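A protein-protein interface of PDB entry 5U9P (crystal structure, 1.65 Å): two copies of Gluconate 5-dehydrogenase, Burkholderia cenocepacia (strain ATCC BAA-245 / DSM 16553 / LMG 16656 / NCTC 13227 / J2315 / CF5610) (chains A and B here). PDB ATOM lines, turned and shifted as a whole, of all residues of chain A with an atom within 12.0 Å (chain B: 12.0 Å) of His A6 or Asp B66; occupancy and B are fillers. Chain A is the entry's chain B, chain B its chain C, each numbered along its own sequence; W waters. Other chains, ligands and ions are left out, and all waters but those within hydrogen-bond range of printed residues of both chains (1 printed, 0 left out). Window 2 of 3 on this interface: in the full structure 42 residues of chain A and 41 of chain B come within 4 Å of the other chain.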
ATOM      1  N   HIS A   5      18.332  -2.712 -31.712  1.00  0.00           N
ATOM      2  CA  HIS A   5      18.834  -3.897 -32.399  1.00  0.00           C
ATOM      3  C   HIS A   5      19.086  -5.033 -31.411  1.00  0.00           C
ATOM      4  O   HIS A   5      18.357  -6.019 -31.395  1.00  0.00           O
ATOM      5  CB  HIS A   5      20.115  -3.572 -33.174  1.00  0.00           C
ATOM      6  N   HIS A   6      20.117  -4.897 -30.581  1.00  0.00           N
ATOM      7  CA  HIS A   6      20.429  -5.952 -29.630  1.00  0.00           C
ATOM      8  C   HIS A   6      19.395  -5.971 -28.505  1.00  0.00           C
ATOM      9  O   HIS A   6      18.655  -5.008 -28.288  1.00  0.00           O
ATOM     10  CB  HIS A   6      21.833  -5.764 -29.059  1.00  0.00           C
ATOM     11  CG  HIS A   6      22.896  -5.645 -30.101  1.00  0.00           C
ATOM     12  ND1 HIS A   6      24.035  -4.890 -29.918  1.00  0.00           N
ATOM     13  CD2 HIS A   6      22.986  -6.171 -31.346  1.00  0.00           C
ATOM     14  CE1 HIS A   6      24.784  -4.961 -31.006  1.00  0.00           C
ATOM     15  NE2 HIS A   6      24.171  -5.732 -31.889  1.00  0.00           N
ATOM     16  N   HIS A   7      19.346  -7.093 -27.787  1.00  0.00           N
ATOM     17  CA  HIS A   7      18.394  -7.287 -26.701  1.00  0.00           C
ATOM     18  C   HIS A   7      19.131  -7.912 -25.531  1.00  0.00           C
ATOM     19  O   HIS A   7      19.664  -9.019 -25.655  1.00  0.00           O
ATOM     20  CB  HIS A   7      17.224  -8.183 -27.129  1.00  0.00           C
ATOM     21  CG  HIS A   7      16.519  -7.710 -28.360  1.00  0.00           C
ATOM     22  ND1 HIS A   7      16.847  -8.158 -29.623  1.00  0.00           N
ATOM     23  CD2 HIS A   7      15.519  -6.812 -28.528  1.00  0.00           C
ATOM     24  CE1 HIS A   7      16.071  -7.561 -30.514  1.00  0.00           C
ATOM     25  NE2 HIS A   7      15.260  -6.738 -29.876  1.00  0.00           N
ATOM     26  N   HIS A   8      19.161  -7.219 -24.396  1.00  0.00           N
ATOM     27  CA  HIS A   8      19.753  -7.809 -23.206  1.00  0.00           C
ATOM     28  C   HIS A   8      18.811  -8.864 -22.631  1.00  0.00           C
ATOM     29  O   HIS A   8      17.610  -8.618 -22.471  1.00  0.00           O
ATOM     30  CB  HIS A   8      20.070  -6.748 -22.158  1.00  0.00           C
ATOM     31  CG  HIS A   8      20.788  -7.297 -20.965  1.00  0.00           C
ATOM     32  ND1 HIS A   8      20.126  -7.847 -19.887  1.00  0.00           N
ATOM     33  CD2 HIS A   8      22.109  -7.414 -20.697  1.00  0.00           C
ATOM     34  CE1 HIS A   8      21.010  -8.262 -18.996  1.00  0.00           C
ATOM     35  NE2 HIS A   8      22.220  -8.012 -19.463  1.00  0.00           N
ATOM     36  N   MET A   9      19.359 -10.042 -22.334  1.00  0.00           N
ATOM     37  CA  MET A   9      18.601 -11.168 -21.814  1.00  0.00           C
ATOM     38  C   MET A   9      19.227 -11.636 -20.501  1.00  0.00           C
ATOM     39  O   MET A   9      20.365 -11.297 -20.173  1.00  0.00           O
ATOM     40  CB  MET A   9      18.531 -12.313 -22.835  1.00  0.00           C
ATOM     41  CG  MET A   9      18.047 -11.896 -24.230  1.00  0.00           C
ATOM     42  SD  MET A   9      16.282 -11.496 -24.309  1.00  0.00           S
ATOM     43  CE  MET A   9      15.542 -13.087 -23.937  1.00  0.00           C
ATOM     44  N   THR A  10      18.463 -12.434 -19.757  1.00  0.00           N
ATOM     45  CA  THR A  10      18.651 -12.576 -18.316  1.00  0.00           C
ATOM     46  C   THR A  10      18.664 -14.034 -17.854  1.00  0.00           C
ATOM     47  O   THR A  10      18.315 -14.322 -16.701  1.00  0.00           O
ATOM     48  CB  THR A  10      17.554 -11.811 -17.576  1.00  0.00           C
ATOM     49  OG1 THR A  10      16.271 -12.225 -18.078  1.00  0.00           O
ATOM     50  CG2 THR A  10      17.716 -10.296 -17.779  1.00  0.00           C
ATOM     51  N   HIS A  11      19.102 -14.960 -18.717  1.00  0.00           N
ATOM     52  CA  HIS A  11      18.881 -16.388 -18.471  1.00  0.00           C
ATOM     53  C   HIS A  11      19.386 -16.838 -17.096  1.00  0.00           C
ATOM     54  O   HIS A  11      18.671 -17.522 -16.354  1.00  0.00           O
ATOM     55  CB  HIS A  11      19.539 -17.214 -19.584  1.00  0.00           C
ATOM     56  CG  HIS A  11      19.069 -16.856 -20.965  1.00  0.00           C
ATOM     57  ND1 HIS A  11      17.848 -17.261 -21.468  1.00  0.00           N
ATOM     58  CD2 HIS A  11      19.659 -16.134 -21.950  1.00  0.00           C
ATOM     59  CE1 HIS A  11      17.705 -16.801 -22.700  1.00  0.00           C
ATOM     60  NE2 HIS A  11      18.789 -16.112 -23.015  1.00  0.00           N
ATOM     61  N   ARG B  38      29.532 -14.307 -18.714  1.00  0.00           N
ATOM     62  CA  ARG B  38      28.224 -14.276 -19.370  1.00  0.00           C
ATOM     63  C   ARG B  38      27.098 -14.258 -18.342  1.00  0.00           C
ATOM     64  O   ARG B  38      26.098 -13.540 -18.507  1.00  0.00           O
ATOM     65  CB  ARG B  38      28.074 -15.475 -20.312  1.00  0.00           C
ATOM     66  CG  ARG B  38      26.920 -15.310 -21.301  1.00  0.00           C
ATOM     67  CD  ARG B  38      26.717 -16.569 -22.169  1.00  0.00           C
ATOM     68  NE  ARG B  38      27.886 -16.939 -22.980  1.00  0.00           N
ATOM     69  CZ  ARG B  38      28.683 -17.972 -22.713  1.00  0.00           C
ATOM     70  NH1 ARG B  38      28.450 -18.727 -21.645  1.00  0.00           N
ATOM     71  NH2 ARG B  38      29.710 -18.257 -23.509  1.00  0.00           N
ATOM     72  N   ALA B  41      26.806 -10.826 -16.672  1.00  0.00           N
ATOM     73  CA  ALA B  41      26.209  -9.892 -17.625  1.00  0.00           C
ATOM     74  C   ALA B  41      24.715 -10.128 -17.755  1.00  0.00           C
ATOM     75  O   ALA B  41      23.938  -9.168 -17.840  1.00  0.00           O
ATOM     76  CB  ALA B  41      26.881  -9.999 -19.000  1.00  0.00           C
ATOM     77  N   GLU B  42      24.283 -11.403 -17.755  1.00  0.00           N
ATOM     78  CA  GLU B  42      22.849 -11.672 -17.866  1.00  0.00           C
ATOM     79  C   GLU B  42      22.090 -11.169 -16.647  1.00  0.00           C
ATOM     80  O   GLU B  42      20.906 -10.806 -16.758  1.00  0.00           O
ATOM     81  CB  GLU B  42      22.613 -13.170 -18.080  1.00  0.00           C
ATOM     82  CG  GLU B  42      22.977 -13.633 -19.485  1.00  0.00           C
ATOM     83  CD  GLU B  42      22.912 -15.149 -19.639  1.00  0.00           C
ATOM     84  OE1 GLU B  42      22.700 -15.828 -18.619  1.00  0.00           O
ATOM     85  OE2 GLU B  42      23.069 -15.660 -20.773  1.00  0.00           O
ATOM     86  N   ILE B  47      30.547  -6.044 -17.843  1.00  0.00           N
ATOM     87  CA  ILE B  47      31.626  -6.980 -17.537  1.00  0.00           C
ATOM     88  C   ILE B  47      32.935  -6.541 -18.196  1.00  0.00           C
ATOM     89  O   ILE B  47      32.977  -5.707 -19.106  1.00  0.00           O
ATOM     90  CB  ILE B  47      31.274  -8.460 -17.887  1.00  0.00           C
ATOM     91  CG1 ILE B  47      30.972  -8.685 -19.369  1.00  0.00           C
ATOM     92  CG2 ILE B  47      30.080  -8.963 -17.078  1.00  0.00           C
ATOM     93  CD1 ILE B  47      32.234  -8.969 -20.221  1.00  0.00           C
ATOM     94  N   ILE B  49      36.373  -8.455 -19.700  1.00  0.00           N
ATOM     95  CA  ILE B  49      37.139  -9.632 -20.091  1.00  0.00           C
ATOM     96  C   ILE B  49      38.606  -9.363 -19.815  1.00  0.00           C
ATOM     97  O   ILE B  49      39.120  -8.298 -20.179  1.00  0.00           O
ATOM     98  CB  ILE B  49      36.920  -9.943 -21.583  1.00  0.00           C
ATOM     99  CG1 ILE B  49      35.434 -10.220 -21.869  1.00  0.00           C
ATOM    100  CG2 ILE B  49      37.810 -11.127 -22.029  1.00  0.00           C
ATOM    101  CD1 ILE B  49      34.878 -11.461 -21.124  1.00  0.00           C
ATOM    102  N   GLU B  55      44.392  -8.749 -28.247  1.00  0.00           N
ATOM    103  CA  GLU B  55      43.456  -8.995 -29.338  1.00  0.00           C
ATOM    104  C   GLU B  55      42.379  -9.977 -28.905  1.00  0.00           C
ATOM    105  O   GLU B  55      41.191  -9.763 -29.157  1.00  0.00           O
ATOM    106  CB  GLU B  55      44.191  -9.506 -30.583  1.00  0.00           C
ATOM    107  CG  GLU B  55      43.221  -9.745 -31.754  1.00  0.00           C
ATOM    108  CD  GLU B  55      43.913 -10.217 -33.027  1.00  0.00           C
ATOM    109  OE1 GLU B  55      45.142 -10.378 -33.020  1.00  0.00           O
ATOM    110  OE2 GLU B  55      43.209 -10.442 -34.033  1.00  0.00           O
ATOM    111  N   LYS B  56      42.761 -11.022 -28.171  1.00  0.00           N
ATOM    112  CA  LYS B  56      41.753 -11.985 -27.752  1.00  0.00           C
ATOM    113  C   LYS B  56      40.753 -11.352 -26.783  1.00  0.00           C
ATOM    114  O   LYS B  56      39.537 -11.511 -26.943  1.00  0.00           O
ATOM    115  CB  LYS B  56      42.422 -13.216 -27.129  1.00  0.00           C
ATOM    116  CG  LYS B  56      41.393 -14.305 -26.804  1.00  0.00           C
ATOM    117  CD  LYS B  56      42.001 -15.642 -26.359  1.00  0.00           C
ATOM    118  CE  LYS B  56      40.864 -16.661 -26.158  1.00  0.00           C
ATOM    119  NZ  LYS B  56      41.366 -18.014 -25.836  1.00  0.00           N
ATOM    120  N   ALA B  57      41.247 -10.627 -25.770  1.00  0.00           N
ATOM    121  CA  ALA B  57      40.355 -10.010 -24.795  1.00  0.00           C
ATOM    122  C   ALA B  57      39.431  -8.998 -25.462  1.00  0.00           C
ATOM    123  O   ALA B  57      38.224  -8.976 -25.199  1.00  0.00           O
ATOM    124  CB  ALA B  57      41.163  -9.340 -23.683  1.00  0.00           C
ATOM    125  N   ALA B  58      39.994  -8.126 -26.301  1.00  0.00           N
ATOM    126  CA  ALA B  58      39.196  -7.074 -26.917  1.00  0.00           C
ATOM    127  C   ALA B  58      38.174  -7.658 -27.887  1.00  0.00           C
ATOM    128  O   ALA B  58      37.055  -7.150 -28.003  1.00  0.00           O
ATOM    129  CB  ALA B  58      40.120  -6.078 -27.630  1.00  0.00           C
ATOM    130  N   THR B  59      38.539  -8.711 -28.598  1.00  0.00           N
ATOM    131  CA  THR B  59      37.598  -9.298 -29.554  1.00  0.00           C
ATOM    132  C   THR B  59      36.462 -10.016 -28.831  1.00  0.00           C
ATOM    133  O   THR B  59      35.302  -9.951 -29.258  1.00  0.00           O
ATOM    134  CB  THR B  59      38.332 -10.251 -30.504  1.00  0.00           C
ATOM    135  OG1 THR B  59      39.279  -9.503 -31.283  1.00  0.00           O
ATOM    136  CG2 THR B  59      37.327 -10.953 -31.450  1.00  0.00           C
ATOM    137  N   LEU B  60      36.775 -10.713 -27.737  1.00  0.00           N
ATOM    138  CA  LEU B  60      35.722 -11.328 -26.931  1.00  0.00           C
ATOM    139  C   LEU B  60      34.786 -10.267 -26.344  1.00  0.00           C
ATOM    140  O   LEU B  60      33.559 -10.438 -26.362  1.00  0.00           O
ATOM    141  CB  LEU B  60      36.351 -12.190 -25.830  1.00  0.00           C
ATOM    142  CG  LEU B  60      35.322 -12.987 -25.024  1.00  0.00           C
ATOM    143  CD1 LEU B  60      34.416 -13.826 -25.933  1.00  0.00           C
ATOM    144  CD2 LEU B  60      36.031 -13.876 -23.988  1.00  0.00           C
ATOM    145  N   ALA B  61      35.342  -9.159 -25.837  1.00  0.00           N
ATOM    146  CA  ALA B  61      34.482  -8.088 -25.339  1.00  0.00           C
ATOM    147  C   ALA B  61      33.568  -7.577 -26.442  1.00  0.00           C
ATOM    148  O   ALA B  61      32.384  -7.307 -26.202  1.00  0.00           O
ATOM    149  CB  ALA B  61      35.309  -6.936 -24.754  1.00  0.00           C
ATOM    150  N   ARG B  62      34.100  -7.423 -27.661  1.00  0.00           N
ATOM    151  CA  ARG B  62      33.264  -6.998 -28.785  1.00  0.00           C
ATOM    152  C   ARG B  62      32.119  -7.977 -29.028  1.00  0.00           C
ATOM    153  O   ARG B  62      30.980  -7.566 -29.293  1.00  0.00           O
ATOM    154  CB  ARG B  62      34.125  -6.856 -30.041  1.00  0.00           C
ATOM    155  CG  ARG B  62      33.328  -6.658 -31.340  1.00  0.00           C
ATOM    156  CD  ARG B  62      32.459  -5.399 -31.288  1.00  0.00           C
ATOM    157  NE  ARG B  62      31.584  -5.323 -32.455  1.00  0.00           N
ATOM    158  CZ  ARG B  62      31.637  -4.372 -33.384  1.00  0.00           C
ATOM    159  NH1 ARG B  62      32.520  -3.388 -33.288  1.00  0.00           N
ATOM    160  NH2 ARG B  62      30.793  -4.403 -34.404  1.00  0.00           N
ATOM    161  N   ARG B  63      32.398  -9.285 -28.954  1.00  0.00           N
ATOM    162  CA  ARG B  63      31.319 -10.259 -29.155  1.00  0.00           C
ATOM    163  C   ARG B  63      30.254 -10.185 -28.060  1.00  0.00           C
ATOM    164  O   ARG B  63      29.067 -10.416 -28.346  1.00  0.00           O
ATOM    165  CB  ARG B  63      31.879 -11.682 -29.269  1.00  0.00           C
ATOM    166  CG  ARG B  63      32.747 -11.804 -30.524  1.00  0.00           C
ATOM    167  CD  ARG B  63      33.484 -13.146 -30.692  1.00  0.00           C
ATOM    168  NE  ARG B  63      34.219 -13.067 -31.957  1.00  0.00           N
ATOM    169  CZ  ARG B  63      35.299 -13.772 -32.273  1.00  0.00           C
ATOM    170  NH1 ARG B  63      35.801 -14.669 -31.437  1.00  0.00           N
ATOM    171  NH2 ARG B  63      35.882 -13.559 -33.449  1.00  0.00           N
ATOM    172  N   PHE B  64      30.641  -9.865 -26.824  1.00  0.00           N
ATOM    173  CA  PHE B  64      29.658  -9.580 -25.780  1.00  0.00           C
ATOM    174  C   PHE B  64      28.830  -8.349 -26.131  1.00  0.00           C
ATOM    175  O   PHE B  64      27.615  -8.332 -25.919  1.00  0.00           O
ATOM    176  CB  PHE B  64      30.356  -9.346 -24.429  1.00  0.00           C
ATOM    177  CG  PHE B  64      30.613 -10.599 -23.606  1.00  0.00           C
ATOM    178  CD1 PHE B  64      29.871 -10.841 -22.457  1.00  0.00           C
ATOM    179  CD2 PHE B  64      31.611 -11.490 -23.951  1.00  0.00           C
ATOM    180  CE1 PHE B  64      30.110 -11.973 -21.668  1.00  0.00           C
ATOM    181  CE2 PHE B  64      31.856 -12.622 -23.174  1.00  0.00           C
ATOM    182  CZ  PHE B  64      31.095 -12.868 -22.040  1.00  0.00           C
ATOM    183  N   ARG B  65      29.467  -7.296 -26.660  1.00  0.00           N
ATOM    184  CA  ARG B  65      28.709  -6.090 -26.972  1.00  0.00           C
ATOM    185  C   ARG B  65      27.737  -6.339 -28.118  1.00  0.00           C
ATOM    186  O   ARG B  65      26.630  -5.793 -28.126  1.00  0.00           O
ATOM    187  CB  ARG B  65      29.656  -4.922 -27.312  1.00  0.00           C
ATOM    188  CG  ARG B  65      30.441  -4.395 -26.093  1.00  0.00           C
ATOM    189  CD  ARG B  65      31.119  -3.056 -26.374  1.00  0.00           C
ATOM    190  NE  ARG B  65      32.081  -3.144 -27.464  1.00  0.00           N
ATOM    191  CZ  ARG B  65      33.360  -3.510 -27.343  1.00  0.00           C
ATOM    192  NH1 ARG B  65      33.870  -3.855 -26.152  1.00  0.00           N
ATOM    193  NH2 ARG B  65      34.146  -3.512 -28.434  1.00  0.00           N
ATOM    194  N   ASP B  66      28.151  -7.146 -29.104  1.00  0.00           N
ATOM    195  CA  ASP B  66      27.242  -7.554 -30.172  1.00  0.00           C
ATOM    196  C   ASP B  66      25.998  -8.254 -29.621  1.00  0.00           C
ATOM    197  O   ASP B  66      24.922  -8.151 -30.224  1.00  0.00           O
ATOM    198  CB  ASP B  66      27.961  -8.480 -31.158  1.00  0.00           C
ATOM    199  CG  ASP B  66      29.052  -7.773 -31.945  1.00  0.00           C
ATOM    200  OD1 ASP B  66      29.019  -6.521 -32.025  1.00  0.00           O
ATOM    201  OD2 ASP B  66      29.907  -8.492 -32.523  1.00  0.00           O
ATOM    202  N   GLU B  67      26.121  -8.947 -28.488  1.00  0.00           N
ATOM    203  CA  GLU B  67      24.993  -9.612 -27.850  1.00  0.00           C
ATOM    204  C   GLU B  67      24.281  -8.717 -26.831  1.00  0.00           C
ATOM    205  O   GLU B  67      23.557  -9.225 -25.967  1.00  0.00           O
ATOM    206  CB  GLU B  67      25.457 -10.927 -27.204  1.00  0.00           C
ATOM    207  CG  GLU B  67      25.708 -12.026 -28.268  1.00  0.00           C
ATOM    208  CD  GLU B  67      26.159 -13.349 -27.703  1.00  0.00           C
ATOM    209  OE1 GLU B  67      26.072 -13.567 -26.473  1.00  0.00           O
ATOM    210  OE2 GLU B  67      26.590 -14.188 -28.519  1.00  0.00           O
ATOM    211  N   GLY B  68      24.479  -7.403 -26.904  1.00  0.00           N
ATOM    212  CA  GLY B  68      23.681  -6.495 -26.104  1.00  0.00           C
ATOM    213  C   GLY B  68      24.169  -6.305 -24.689  1.00  0.00           C
ATOM    214  O   GLY B  68      23.456  -5.699 -23.881  1.00  0.00           O
ATOM    215  N   PHE B  69      25.360  -6.801 -24.359  1.00  0.00           N
ATOM    216  CA  PHE B  69      25.921  -6.639 -23.028  1.00  0.00           C
ATOM    217  C   PHE B  69      26.852  -5.432 -23.004  1.00  0.00           C
ATOM    218  O   PHE B  69      27.482  -5.089 -24.008  1.00  0.00           O
ATOM    219  CB  PHE B  69      26.716  -7.881 -22.606  1.00  0.00           C
ATOM    220  CG  PHE B  69      25.909  -9.146 -22.569  1.00  0.00           C
ATOM    221  CD1 PHE B  69      24.853  -9.290 -21.675  1.00  0.00           C
ATOM    222  CD2 PHE B  69      26.232 -10.215 -23.411  1.00  0.00           C
ATOM    223  CE1 PHE B  69      24.130 -10.485 -21.609  1.00  0.00           C
ATOM    224  CE2 PHE B  69      25.508 -11.412 -23.363  1.00  0.00           C
ATOM    225  CZ  PHE B  69      24.453 -11.547 -22.471  1.00  0.00           C
ATOM    226  N   ALA B  70      26.924  -4.774 -21.859  1.00  0.00           N
ATOM    227  CA  ALA B  70      27.979  -3.788 -21.660  1.00  0.00           C
ATOM    228  C   ALA B  70      29.262  -4.533 -21.325  1.00  0.00           C
ATOM    229  O   ALA B  70      29.292  -5.341 -20.388  1.00  0.00           O
ATOM    230  CB  ALA B  70      27.616  -2.813 -20.542  1.00  0.00           C
ATOM    231  N   ALA B  71      30.319  -4.281 -22.094  1.00  0.00           N
ATOM    232  CA  ALA B  71      31.518  -5.095 -21.942  1.00  0.00           C
ATOM    233  C   ALA B  71      32.742  -4.319 -22.394  1.00  0.00           C
ATOM    234  O   ALA B  71      32.698  -3.615 -23.409  1.00  0.00           O
ATOM    235  CB  ALA B  71      31.413  -6.403 -22.741  1.00  0.00           C
ATOM    236  N   ASP B  72      33.831  -4.466 -21.627  1.00  0.00           N
ATOM    237  CA  ASP B  72      35.128  -3.868 -21.939  1.00  0.00           C
ATOM    238  C   ASP B  72      36.200  -4.929 -21.680  1.00  0.00           C
ATOM    239  O   ASP B  72      35.896  -6.084 -21.361  1.00  0.00           O
ATOM    240  CB  ASP B  72      35.350  -2.622 -21.085  1.00  0.00           C
ATOM    241  CG  ASP B  72      34.462  -1.486 -21.467  1.00  0.00           C
ATOM    242  OD1 ASP B  72      34.867  -0.680 -22.348  1.00  0.00           O
ATOM    243  OD2 ASP B  72      33.364  -1.396 -20.867  1.00  0.00           O
HETATM  244  O   HOH W   1      21.467 -10.755 -24.001  1.00  0.00           O
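N of Phe B69 is in hydrogen-bond range of O of Phe B64 (3.1 Å).
The guanidinium group (NE) of Arg B62 is in salt-bridge range of the side-chain carboxylate (OD1) of Asp B66, at 2.9 Å.
ND1 of His A7 sits close to O of His A5.
The backbone carbonyl oxygen of Ala B71 is in hydrogen-bond range of the guanidinium group of Arg B65 (3.0 Å).
No position is printed for both chains.
Of the 11 pairs that touch across the chains among the printed residues, none has its exchanged pair printed and touching as well.
Among the printed residues, pairs that only touch across the chains: His A6 with Gly B68 (3.6 Å), His A7 with Glu B67 (3.9 Å), His A8 with Glu B42 (3.4 Å), His A8 with Gly B68 (3.9 Å), His A8 with Phe B69 (3.5 Å), Thr A10 with Glu B42 (3.3 Å) and His A11 with Glu B42 (3.6 Å).
Of the 23 printed residues of chain B, 7 touch a printed residue of chain A.
Hydrophobic or aromatic side chains of chain B that line the printed part of chain A: Phe B69.
Along chain B the printed residues that touch a printed residue of chain A span positions 41 to 69.
Of the 7 printed residues of chain A, 6 touch a printed residue of chain B.
Hydrophobic or aromatic side chains of chain A within 4 Å of the printed part of chain B: His A6, His A8 and His A11.
Among the printed residues, 11 pairs touch across the chains.
No residue of chain B comes within 4 Å of His A5.
His A6 touches just these residues of chain B: Arg B65, Asp B66 and Gly B68.
Printed residues of chain B within 4 Å of Met A9: Glu B42.
Printed residues of chain B within 4 Å of His A11: Glu B42.
Of the printed residues of chain A, Ala B41 touches His A8 (2.6 Å).
Printed residues of chain A within 4 Å of Arg B65: His A6 (3.3 Å).
Asp B66 touches one residue of chain A.
Of chain A, only His A7 (3.9 Å) comes within 4 Å of Glu B67.
Gly B68 touches just these residues of chain A: His A6 and His A8.
Printed residues of chain A within 4 Å of Phe B69: His A8 (3.5 Å).
The nearest residue of chain B that does not touch His A6 is Glu B67 (4.4 Å).
The nearest residue of chain A that does not touch Asp B66 is His A7 (6.2 Å).
Water W1 lies within hydrogen-bond range of the backbone NH (N) of Met A9 (2.8 Å), the backbone carbonyl oxygen (O) of His A7 (3.0 Å) and the backbone carbonyl oxygen (O) of Glu B67 (3.3 Å).
NE2 of His A8 is in hydrogen-bond range of O of Ala B41 (2.6 Å).
A ring nitrogen (NE2) of His A6 sits close to the backbone carbonyl oxygen of Asp B66 (3.0 Å).
ND1 of His A6 lies within hydrogen-bond range of O of Arg B65, at 3.3 Å.
O of Glu B42 sits close to O of Met A9 (3.5 Å).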
